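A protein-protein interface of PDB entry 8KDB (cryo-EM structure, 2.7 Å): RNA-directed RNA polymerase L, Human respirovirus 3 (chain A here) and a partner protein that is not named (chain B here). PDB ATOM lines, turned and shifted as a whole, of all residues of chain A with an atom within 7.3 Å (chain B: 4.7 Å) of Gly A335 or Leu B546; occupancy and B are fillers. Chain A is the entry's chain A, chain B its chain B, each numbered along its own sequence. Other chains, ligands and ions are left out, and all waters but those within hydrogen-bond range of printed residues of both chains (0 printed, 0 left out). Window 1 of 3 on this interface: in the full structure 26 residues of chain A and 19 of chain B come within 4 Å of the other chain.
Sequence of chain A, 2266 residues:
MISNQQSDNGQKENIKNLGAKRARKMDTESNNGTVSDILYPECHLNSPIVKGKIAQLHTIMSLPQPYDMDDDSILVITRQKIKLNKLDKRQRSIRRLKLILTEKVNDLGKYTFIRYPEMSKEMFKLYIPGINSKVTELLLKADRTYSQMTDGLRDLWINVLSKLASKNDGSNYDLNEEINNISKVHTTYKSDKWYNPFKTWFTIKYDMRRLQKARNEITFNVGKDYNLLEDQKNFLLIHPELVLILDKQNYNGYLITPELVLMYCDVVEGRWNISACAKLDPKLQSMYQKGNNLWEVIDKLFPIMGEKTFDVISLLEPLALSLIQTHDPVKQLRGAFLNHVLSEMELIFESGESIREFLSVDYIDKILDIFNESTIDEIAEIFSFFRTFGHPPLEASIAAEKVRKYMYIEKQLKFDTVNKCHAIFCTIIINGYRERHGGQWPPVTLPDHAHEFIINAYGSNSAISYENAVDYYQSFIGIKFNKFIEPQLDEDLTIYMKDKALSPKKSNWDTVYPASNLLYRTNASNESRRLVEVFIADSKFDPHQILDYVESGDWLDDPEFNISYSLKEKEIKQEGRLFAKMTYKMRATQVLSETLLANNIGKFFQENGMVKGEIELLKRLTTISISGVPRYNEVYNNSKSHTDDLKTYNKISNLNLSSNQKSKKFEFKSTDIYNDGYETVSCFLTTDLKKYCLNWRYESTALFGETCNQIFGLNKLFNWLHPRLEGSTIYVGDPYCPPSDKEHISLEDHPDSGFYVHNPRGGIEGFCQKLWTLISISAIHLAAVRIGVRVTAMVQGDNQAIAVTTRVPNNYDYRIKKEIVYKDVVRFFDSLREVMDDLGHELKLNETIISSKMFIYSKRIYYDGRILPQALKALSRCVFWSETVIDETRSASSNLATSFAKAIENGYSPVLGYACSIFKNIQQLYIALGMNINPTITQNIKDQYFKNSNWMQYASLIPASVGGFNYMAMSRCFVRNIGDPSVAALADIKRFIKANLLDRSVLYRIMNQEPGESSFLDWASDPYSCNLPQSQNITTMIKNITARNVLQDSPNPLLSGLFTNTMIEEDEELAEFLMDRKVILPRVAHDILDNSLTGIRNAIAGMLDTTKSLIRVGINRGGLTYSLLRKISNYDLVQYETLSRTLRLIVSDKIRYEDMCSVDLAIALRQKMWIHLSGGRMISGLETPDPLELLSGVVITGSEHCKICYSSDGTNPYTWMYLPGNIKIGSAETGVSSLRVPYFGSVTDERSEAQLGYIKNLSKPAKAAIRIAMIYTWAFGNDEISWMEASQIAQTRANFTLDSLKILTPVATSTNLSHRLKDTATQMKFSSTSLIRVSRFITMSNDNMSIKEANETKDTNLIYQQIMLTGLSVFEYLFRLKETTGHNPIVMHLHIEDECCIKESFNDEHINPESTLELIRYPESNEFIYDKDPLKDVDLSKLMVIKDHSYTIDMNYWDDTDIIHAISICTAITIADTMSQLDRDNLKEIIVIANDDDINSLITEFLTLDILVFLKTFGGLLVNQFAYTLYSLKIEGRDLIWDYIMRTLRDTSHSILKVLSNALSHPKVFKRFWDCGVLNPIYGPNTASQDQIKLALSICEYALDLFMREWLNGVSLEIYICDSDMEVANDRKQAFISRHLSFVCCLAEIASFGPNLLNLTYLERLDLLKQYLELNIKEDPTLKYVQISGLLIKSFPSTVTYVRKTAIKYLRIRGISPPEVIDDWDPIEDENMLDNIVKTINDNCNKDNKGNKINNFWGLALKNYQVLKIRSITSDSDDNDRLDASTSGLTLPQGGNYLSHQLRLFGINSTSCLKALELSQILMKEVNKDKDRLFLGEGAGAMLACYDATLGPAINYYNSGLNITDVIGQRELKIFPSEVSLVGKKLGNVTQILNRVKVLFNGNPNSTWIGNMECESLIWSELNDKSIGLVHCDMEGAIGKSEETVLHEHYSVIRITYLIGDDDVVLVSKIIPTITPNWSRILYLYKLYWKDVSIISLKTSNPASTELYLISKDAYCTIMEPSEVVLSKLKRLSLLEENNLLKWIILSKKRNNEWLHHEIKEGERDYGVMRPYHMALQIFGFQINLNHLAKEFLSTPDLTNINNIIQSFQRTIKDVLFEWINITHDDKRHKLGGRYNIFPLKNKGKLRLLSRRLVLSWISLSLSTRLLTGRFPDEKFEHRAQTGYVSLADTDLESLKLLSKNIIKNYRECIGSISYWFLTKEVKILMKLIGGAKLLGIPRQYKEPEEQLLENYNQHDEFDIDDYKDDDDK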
ATOM      1  N   SER A 322      16.556  25.154   6.148  1.00  0.00           N
ATOM      2  CA  SER A 322      17.690  24.538   6.830  1.00  0.00           C
ATOM      3  C   SER A 322      17.632  23.016   6.752  1.00  0.00           C
ATOM      4  O   SER A 322      18.664  22.357   6.560  1.00  0.00           O
ATOM      5  CB  SER A 322      17.733  24.998   8.285  1.00  0.00           C
ATOM      6  OG  SER A 322      16.605  24.530   9.000  1.00  0.00           O
ATOM      7  N   GLN A 325      18.810  22.040   3.517  1.00  0.00           N
ATOM      8  CA  GLN A 325      20.246  22.276   3.419  1.00  0.00           C
ATOM      9  C   GLN A 325      21.075  21.201   4.110  1.00  0.00           C
ATOM     10  O   GLN A 325      22.222  20.977   3.714  1.00  0.00           O
ATOM     11  CB  GLN A 325      20.595  23.643   4.008  1.00  0.00           C
ATOM     12  CG  GLN A 325      22.006  24.109   3.705  1.00  0.00           C
ATOM     13  CD  GLN A 325      22.483  25.175   4.666  1.00  0.00           C
ATOM     14  OE1 GLN A 325      22.211  25.109   5.863  1.00  0.00           O
ATOM     15  NE2 GLN A 325      23.199  26.164   4.149  1.00  0.00           N
ATOM     16  N   THR A 326      20.530  20.532   5.129  1.00  0.00           N
ATOM     17  CA  THR A 326      21.310  19.500   5.815  1.00  0.00           C
ATOM     18  C   THR A 326      21.689  18.323   4.919  1.00  0.00           C
ATOM     19  O   THR A 326      22.376  17.412   5.391  1.00  0.00           O
ATOM     20  CB  THR A 326      20.565  18.951   7.040  1.00  0.00           C
ATOM     21  OG1 THR A 326      19.442  18.166   6.617  1.00  0.00           O
ATOM     22  CG2 THR A 326      20.110  20.064   7.961  1.00  0.00           C
ATOM     23  N   HIS A 327      21.267  18.309   3.657  1.00  0.00           N
ATOM     24  CA  HIS A 327      21.551  17.205   2.749  1.00  0.00           C
ATOM     25  C   HIS A 327      22.676  17.490   1.758  1.00  0.00           C
ATOM     26  O   HIS A 327      22.927  16.652   0.886  1.00  0.00           O
ATOM     27  CB  HIS A 327      20.292  16.831   1.958  1.00  0.00           C
ATOM     28  CG  HIS A 327      19.244  16.136   2.768  1.00  0.00           C
ATOM     29  ND1 HIS A 327      18.354  16.812   3.574  1.00  0.00           N
ATOM     30  CD2 HIS A 327      18.932  14.824   2.883  1.00  0.00           C
ATOM     31  CE1 HIS A 327      17.545  15.947   4.158  1.00  0.00           C
ATOM     32  NE2 HIS A 327      17.874  14.733   3.755  1.00  0.00           N
ATOM     33  N   ASP A 328      23.358  18.634   1.853  1.00  0.00           N
ATOM     34  CA  ASP A 328      24.230  18.978   0.738  1.00  0.00           C
ATOM     35  C   ASP A 328      25.614  18.336   0.880  1.00  0.00           C
ATOM     36  O   ASP A 328      26.053  18.030   1.992  1.00  0.00           O
ATOM     37  CB  ASP A 328      24.358  20.495   0.605  1.00  0.00           C
ATOM     38  CG  ASP A 328      25.356  21.090   1.567  1.00  0.00           C
ATOM     39  OD1 ASP A 328      25.469  20.601   2.709  1.00  0.00           O
ATOM     40  OD2 ASP A 328      26.045  22.047   1.163  1.00  0.00           O
ATOM     41  N   VAL A 330      28.701  19.446   0.591  1.00  0.00           N
ATOM     42  CA  VAL A 330      29.751  20.179   1.289  1.00  0.00           C
ATOM     43  C   VAL A 330      29.524  20.071   2.790  1.00  0.00           C
ATOM     44  O   VAL A 330      28.441  20.389   3.297  1.00  0.00           O
ATOM     45  CB  VAL A 330      29.784  21.643   0.827  1.00  0.00           C
ATOM     46  CG1 VAL A 330      30.824  22.419   1.608  1.00  0.00           C
ATOM     47  CG2 VAL A 330      30.070  21.716  -0.660  1.00  0.00           C
ATOM     48  N   LYS A 331      30.552  19.620   3.511  1.00  0.00           N
ATOM     49  CA  LYS A 331      30.396  19.320   4.929  1.00  0.00           C
ATOM     50  C   LYS A 331      30.270  20.570   5.786  1.00  0.00           C
ATOM     51  O   LYS A 331      29.684  20.502   6.871  1.00  0.00           O
ATOM     52  CB  LYS A 331      31.569  18.470   5.416  1.00  0.00           C
ATOM     53  CG  LYS A 331      32.925  19.129   5.242  1.00  0.00           C
ATOM     54  CD  LYS A 331      34.033  18.267   5.817  1.00  0.00           C
ATOM     55  CE  LYS A 331      35.374  18.974   5.742  1.00  0.00           C
ATOM     56  NZ  LYS A 331      36.503  18.044   6.007  1.00  0.00           N
ATOM     57  N   GLN A 332      30.804  21.705   5.334  1.00  0.00           N
ATOM     58  CA  GLN A 332      30.707  22.928   6.122  1.00  0.00           C
ATOM     59  C   GLN A 332      29.303  23.515   6.116  1.00  0.00           C
ATOM     60  O   GLN A 332      28.953  24.255   7.041  1.00  0.00           O
ATOM     61  CB  GLN A 332      31.699  23.972   5.607  1.00  0.00           C
ATOM     62  CG  GLN A 332      33.153  23.679   5.930  1.00  0.00           C
ATOM     63  CD  GLN A 332      33.816  22.794   4.896  1.00  0.00           C
ATOM     64  OE1 GLN A 332      33.252  22.525   3.838  1.00  0.00           O
ATOM     65  NE2 GLN A 332      35.029  22.347   5.194  1.00  0.00           N
ATOM     66  N   LEU A 333      28.496  23.205   5.106  1.00  0.00           N
ATOM     67  CA  LEU A 333      27.171  23.790   4.960  1.00  0.00           C
ATOM     68  C   LEU A 333      26.061  22.950   5.574  1.00  0.00           C
ATOM     69  O   LEU A 333      24.901  23.373   5.541  1.00  0.00           O
ATOM     70  CB  LEU A 333      26.860  24.029   3.481  1.00  0.00           C
ATOM     71  CG  LEU A 333      27.737  25.034   2.740  1.00  0.00           C
ATOM     72  CD1 LEU A 333      27.357  25.087   1.272  1.00  0.00           C
ATOM     73  CD2 LEU A 333      27.620  26.405   3.376  1.00  0.00           C
ATOM     74  N   ARG A 334      26.370  21.782   6.131  1.00  0.00           N
ATOM     75  CA  ARG A 334      25.340  20.927   6.713  1.00  0.00           C
ATOM     76  C   ARG A 334      24.968  21.459   8.091  1.00  0.00           C
ATOM     77  O   ARG A 334      25.745  21.337   9.044  1.00  0.00           O
ATOM     78  CB  ARG A 334      25.818  19.481   6.798  1.00  0.00           C
ATOM     79  CG  ARG A 334      26.068  18.828   5.454  1.00  0.00           C
ATOM     80  CD  ARG A 334      26.110  17.315   5.576  1.00  0.00           C
ATOM     81  NE  ARG A 334      26.966  16.715   4.562  1.00  0.00           N
ATOM     82  CZ  ARG A 334      28.145  16.164   4.811  1.00  0.00           C
ATOM     83  NH1 ARG A 334      28.634  16.106   6.039  1.00  0.00           N
ATOM     84  NH2 ARG A 334      28.852  15.660   3.805  1.00  0.00           N
ATOM     85  N   GLY A 335      23.779  22.039   8.200  1.00  0.00           N
ATOM     86  CA  GLY A 335      23.304  22.569   9.465  1.00  0.00           C
ATOM     87  C   GLY A 335      23.846  23.933   9.835  1.00  0.00           C
ATOM     88  O   GLY A 335      23.904  24.267  11.024  1.00  0.00           O
ATOM     89  N   ALA A 336      24.248  24.733   8.847  1.00  0.00           N
ATOM     90  CA  ALA A 336      24.710  26.085   9.139  1.00  0.00           C
ATOM     91  C   ALA A 336      23.545  27.030   9.410  1.00  0.00           C
ATOM     92  O   ALA A 336      23.624  27.876  10.306  1.00  0.00           O
ATOM     93  CB  ALA A 336      25.565  26.608   7.987  1.00  0.00           C
ATOM     94  N   PHE A 337      22.465  26.905   8.639  1.00  0.00           N
ATOM     95  CA  PHE A 337      21.265  27.704   8.862  1.00  0.00           C
ATOM     96  C   PHE A 337      20.452  27.187  10.043  1.00  0.00           C
ATOM     97  O   PHE A 337      19.852  27.982  10.784  1.00  0.00           O
ATOM     98  CB  PHE A 337      20.420  27.708   7.586  1.00  0.00           C
ATOM     99  CG  PHE A 337      19.521  28.898   7.450  1.00  0.00           C
ATOM    100  CD1 PHE A 337      20.002  30.177   7.656  1.00  0.00           C
ATOM    101  CD2 PHE A 337      18.194  28.738   7.093  1.00  0.00           C
ATOM    102  CE1 PHE A 337      19.174  31.270   7.524  1.00  0.00           C
ATOM    103  CE2 PHE A 337      17.363  29.829   6.957  1.00  0.00           C
ATOM    104  CZ  PHE A 337      17.854  31.096   7.175  1.00  0.00           C
ATOM    105  N   LEU A 338      20.432  25.865  10.230  1.00  0.00           N
ATOM    106  CA  LEU A 338      19.668  25.270  11.319  1.00  0.00           C
ATOM    107  C   LEU A 338      20.143  25.764  12.676  1.00  0.00           C
ATOM    108  O   LEU A 338      19.333  25.915  13.594  1.00  0.00           O
ATOM    109  CB  LEU A 338      19.760  23.747  11.248  1.00  0.00           C
ATOM    110  CG  LEU A 338      18.884  22.962  12.223  1.00  0.00           C
ATOM    111  CD1 LEU A 338      17.428  23.359  12.078  1.00  0.00           C
ATOM    112  CD2 LEU A 338      19.055  21.473  12.006  1.00  0.00           C
ATOM    113  N   ASN A 339      21.444  26.020  12.822  1.00  0.00           N
ATOM    114  CA  ASN A 339      21.962  26.536  14.085  1.00  0.00           C
ATOM    115  C   ASN A 339      21.306  27.865  14.443  1.00  0.00           C
ATOM    116  O   ASN A 339      20.797  28.042  15.556  1.00  0.00           O
ATOM    117  CB  ASN A 339      23.480  26.687  13.998  1.00  0.00           C
ATOM    118  CG  ASN A 339      24.115  26.991  15.336  1.00  0.00           C
ATOM    119  OD1 ASN A 339      23.438  27.042  16.361  1.00  0.00           O
ATOM    120  ND2 ASN A 339      25.424  27.201  15.334  1.00  0.00           N
ATOM    121  N   HIS A 340      21.295  28.808  13.499  1.00  0.00           N
ATOM    122  CA  HIS A 340      20.689  30.109  13.758  1.00  0.00           C
ATOM    123  C   HIS A 340      19.188  29.987  13.984  1.00  0.00           C
ATOM    124  O   HIS A 340      18.629  30.655  14.866  1.00  0.00           O
ATOM    125  CB  HIS A 340      20.983  31.061  12.600  1.00  0.00           C
ATOM    126  CG  HIS A 340      20.112  32.278  12.584  1.00  0.00           C
ATOM    127  ND1 HIS A 340      18.978  32.370  11.808  1.00  0.00           N
ATOM    128  CD2 HIS A 340      20.212  33.455  13.246  1.00  0.00           C
ATOM    129  CE1 HIS A 340      18.413  33.549  11.997  1.00  0.00           C
ATOM    130  NE2 HIS A 340      19.144  34.227  12.863  1.00  0.00           N
ATOM    131  N   TYR A 822      32.940  25.951  -3.406  1.00  0.00           N
ATOM    132  CA  TYR A 822      32.509  26.478  -2.113  1.00  0.00           C
ATOM    133  C   TYR A 822      33.441  27.578  -1.610  1.00  0.00           C
ATOM    134  O   TYR A 822      32.990  28.547  -0.985  1.00  0.00           O
ATOM    135  CB  TYR A 822      32.415  25.336  -1.101  1.00  0.00           C
ATOM    136  CG  TYR A 822      32.303  25.781   0.336  1.00  0.00           C
ATOM    137  CD1 TYR A 822      31.135  26.356   0.814  1.00  0.00           C
ATOM    138  CD2 TYR A 822      33.359  25.612   1.218  1.00  0.00           C
ATOM    139  CE1 TYR A 822      31.027  26.759   2.125  1.00  0.00           C
ATOM    140  CE2 TYR A 822      33.259  26.014   2.531  1.00  0.00           C
ATOM    141  CZ  TYR A 822      32.091  26.586   2.979  1.00  0.00           C
ATOM    142  OH  TYR A 822      31.988  26.988   4.290  1.00  0.00           O
ATOM    143  N   SER B 541      30.116  30.294  14.289  1.00  0.00           N
ATOM    144  CA  SER B 541      29.294  29.773  13.207  1.00  0.00           C
ATOM    145  C   SER B 541      28.559  30.905  12.503  1.00  0.00           C
ATOM    146  O   SER B 541      28.103  31.861  13.135  1.00  0.00           O
ATOM    147  CB  SER B 541      28.291  28.752  13.743  1.00  0.00           C
ATOM    148  OG  SER B 541      28.947  27.611  14.266  1.00  0.00           O
ATOM    149  N   THR B 544      28.353  30.584   6.346  1.00  0.00           N
ATOM    150  CA  THR B 544      29.324  29.883   5.514  1.00  0.00           C
ATOM    151  C   THR B 544      29.739  28.541   6.101  1.00  0.00           C
ATOM    152  O   THR B 544      30.116  27.636   5.350  1.00  0.00           O
ATOM    153  CB  THR B 544      30.567  30.750   5.304  1.00  0.00           C
ATOM    154  OG1 THR B 544      31.134  31.092   6.573  1.00  0.00           O
ATOM    155  CG2 THR B 544      30.212  32.024   4.566  1.00  0.00           C
ATOM    156  N   ARG B 545      29.680  28.385   7.421  1.00  0.00           N
ATOM    157  CA  ARG B 545      30.203  27.179   8.047  1.00  0.00           C
ATOM    158  C   ARG B 545      29.553  26.977   9.407  1.00  0.00           C
ATOM    159  O   ARG B 545      29.151  27.937  10.068  1.00  0.00           O
ATOM    160  CB  ARG B 545      31.727  27.254   8.194  1.00  0.00           C
ATOM    161  CG  ARG B 545      32.192  28.365   9.119  1.00  0.00           C
ATOM    162  CD  ARG B 545      33.672  28.242   9.452  1.00  0.00           C
ATOM    163  NE  ARG B 545      34.089  29.141  10.525  1.00  0.00           N
ATOM    164  CZ  ARG B 545      33.992  30.465  10.497  1.00  0.00           C
ATOM    165  NH1 ARG B 545      33.549  31.109   9.429  1.00  0.00           N
ATOM    166  NH2 ARG B 545      34.366  31.164  11.565  1.00  0.00           N
ATOM    167  N   LEU B 546      29.460  25.713   9.811  1.00  0.00           N
ATOM    168  CA  LEU B 546      29.003  25.330  11.141  1.00  0.00           C
ATOM    169  C   LEU B 546      30.173  24.701  11.881  1.00  0.00           C
ATOM    170  O   LEU B 546      30.729  23.696  11.427  1.00  0.00           O
ATOM    171  CB  LEU B 546      27.825  24.357  11.064  1.00  0.00           C
ATOM    172  CG  LEU B 546      27.435  23.652  12.365  1.00  0.00           C
ATOM    173  CD1 LEU B 546      26.674  24.594  13.284  1.00  0.00           C
ATOM    174  CD2 LEU B 546      26.616  22.407  12.079  1.00  0.00           C
ATOM    175  N   ILE B 547      30.542  25.287  13.012  1.00  0.00           N
ATOM    176  CA  ILE B 547      31.672  24.826  13.814  1.00  0.00           C
ATOM    177  C   ILE B 547      31.130  23.930  14.922  1.00  0.00           C
ATOM    178  O   ILE B 547      30.316  24.396  15.734  1.00  0.00           O
ATOM    179  CB  ILE B 547      32.466  26.002  14.399  1.00  0.00           C
ATOM    180  CG1 ILE B 547      32.943  26.929  13.281  1.00  0.00           C
ATOM    181  CG2 ILE B 547      33.644  25.495  15.213  1.00  0.00           C
ATOM    182  CD1 ILE B 547      33.749  28.105  13.773  1.00  0.00           C
ATOM    183  N   PRO B 548      31.535  22.661  14.992  1.00  0.00           N
ATOM    184  CA  PRO B 548      31.037  21.776  16.056  1.00  0.00           C
ATOM    185  C   PRO B 548      31.517  22.244  17.422  1.00  0.00           C
ATOM    186  O   PRO B 548      32.715  22.229  17.715  1.00  0.00           O
ATOM    187  CB  PRO B 548      31.626  20.408  15.686  1.00  0.00           C
ATOM    188  CG  PRO B 548      31.996  20.521  14.239  1.00  0.00           C
ATOM    189  CD  PRO B 548      32.401  21.947  14.042  1.00  0.00           C
ATOM    190  N   THR B 554      24.014  24.221  18.601  1.00  0.00           N
ATOM    191  CA  THR B 554      24.852  23.431  17.707  1.00  0.00           C
ATOM    192  C   THR B 554      24.671  21.933  17.910  1.00  0.00           C
ATOM    193  O   THR B 554      24.719  21.176  16.935  1.00  0.00           O
ATOM    194  CB  THR B 554      26.327  23.802  17.894  1.00  0.00           C
ATOM    195  OG1 THR B 554      26.489  25.215  17.720  1.00  0.00           O
ATOM    196  CG2 THR B 554      27.199  23.079  16.882  1.00  0.00           C
ATOM    197  N   SER B 557      21.558  20.882  16.077  1.00  0.00           N
ATOM    198  CA  SER B 557      21.807  20.911  14.640  1.00  0.00           C
ATOM    199  C   SER B 557      22.625  19.705  14.198  1.00  0.00           C
ATOM    200  O   SER B 557      22.348  19.106  13.154  1.00  0.00           O
ATOM    201  CB  SER B 557      22.516  22.209  14.258  1.00  0.00           C
ATOM    202  OG  SER B 557      21.913  23.320  14.894  1.00  0.00           O
ATOM    203  N   LEU B 558      23.641  19.335  14.982  1.00  0.00           N
ATOM    204  CA  LEU B 558      24.445  18.163  14.650  1.00  0.00           C
ATOM    205  C   LEU B 558      23.616  16.887  14.723  1.00  0.00           C
ATOM    206  O   LEU B 558      23.754  16.001  13.869  1.00  0.00           O
ATOM    207  CB  LEU B 558      25.651  18.075  15.584  1.00  0.00           C
ATOM    208  CG  LEU B 558      26.705  19.168  15.414  1.00  0.00           C
ATOM    209  CD1 LEU B 558      27.776  19.046  16.480  1.00  0.00           C
ATOM    210  CD2 LEU B 558      27.316  19.123  14.024  1.00  0.00           C
ATOM    211  N   VAL B 561      21.494  16.784  11.659  1.00  0.00           N
ATOM    212  CA  VAL B 561      22.297  16.460  10.482  1.00  0.00           C
ATOM    213  C   VAL B 561      22.585  14.966  10.431  1.00  0.00           C
ATOM    214  O   VAL B 561      22.484  14.334   9.372  1.00  0.00           O
ATOM    215  CB  VAL B 561      23.595  17.289  10.475  1.00  0.00           C
ATOM    216  CG1 VAL B 561      24.630  16.653   9.561  1.00  0.00           C
ATOM    217  CG2 VAL B 561      23.311  18.716  10.046  1.00  0.00           C
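O of Gln A332 sits at hydrogen-bond distance from N of Leu B546.
The side-chain hydroxyl (OG1) of Thr B554 sits at hydrogen-bond distance from the side-chain amide nitrogen (ND2) of Asn A339 (3.3 Å).
The backbone NH of Asn A339 sits close to the side-chain hydroxyl of Ser B557, at 3.4 Å.
OH of Tyr A822 sits close to O of Thr B544, at 2.2 Å.
The side-chain amide oxygen (OE1) of Gln A325 lies close to the backbone carbonyl oxygen (O) of Leu A333 (3.2 Å).
The backbone carbonyl oxygen (O) of Asp A328 lies within hydrogen-bond range of the guanidinium group (NE) of Arg A334.
N of Ile B547 sits at hydrogen-bond distance from OG of Ser B541 (3.1 Å).
Gln A332 touches Thr B544 (O to O, 3.96 Å).
CA of Arg B545 touches O of Gln A332, at 3.3 Å.
CD2 of Leu B546 touches O of Arg A334, 3.3 Å away.
Arg A334 touches Val B561 (O to CG2, 3.7 Å).
Gly A335 touches Leu B546.
Gly A335 touches Val B561.
C of Leu A338 touches OG of Ser B557 (3.7 Å).
Ser B541 touches Asn A339 (CB to ND2, 3.6 Å).
Asn A339 touches Leu B546 (ND2 to CD1, 3.5 Å).
Tyr A822 touches Arg B545.
Gly A335 touches two residues of chain B.
Of the printed residues of chain B, Leu A338 touches Ser B557 (3.7 Å).
Printed residues of chain A within 4 Å of Ser B557: Leu A338 (3.7 Å) and Asn A339 (3.3 Å).
Of the printed residues of chain A, Ser B541 touches Asn A339.
Of the printed residues of chain B, Asn A339 touches Ser B541 (3.6 Å), Leu B546 (3.5 Å), Thr B554 (3.3 Å) and Ser B557 (3.3 Å).
Of the printed residues of chain B, Leu A333 touches Thr B544 (3.4 Å).
The nearest residue of chain A that does not touch Leu B546 is Ala A336 (4.05 Å).
Of the 10 printed residues of chain B, 7 touch a printed residue of chain A.
Hydrophobic or aromatic side chains of chain A within 4 Å of the printed part of chain B: Leu A333, Leu A338 and Tyr A822.
Along chain A the printed residues that touch a printed residue of chain B span positions 332 to 822.
Among the printed residues, 15 pairs touch across the chains.
Among the printed residues, no Asp or Glu carboxylate lies within 4 Å of a Lys or Arg side-chain nitrogen of the other chain.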
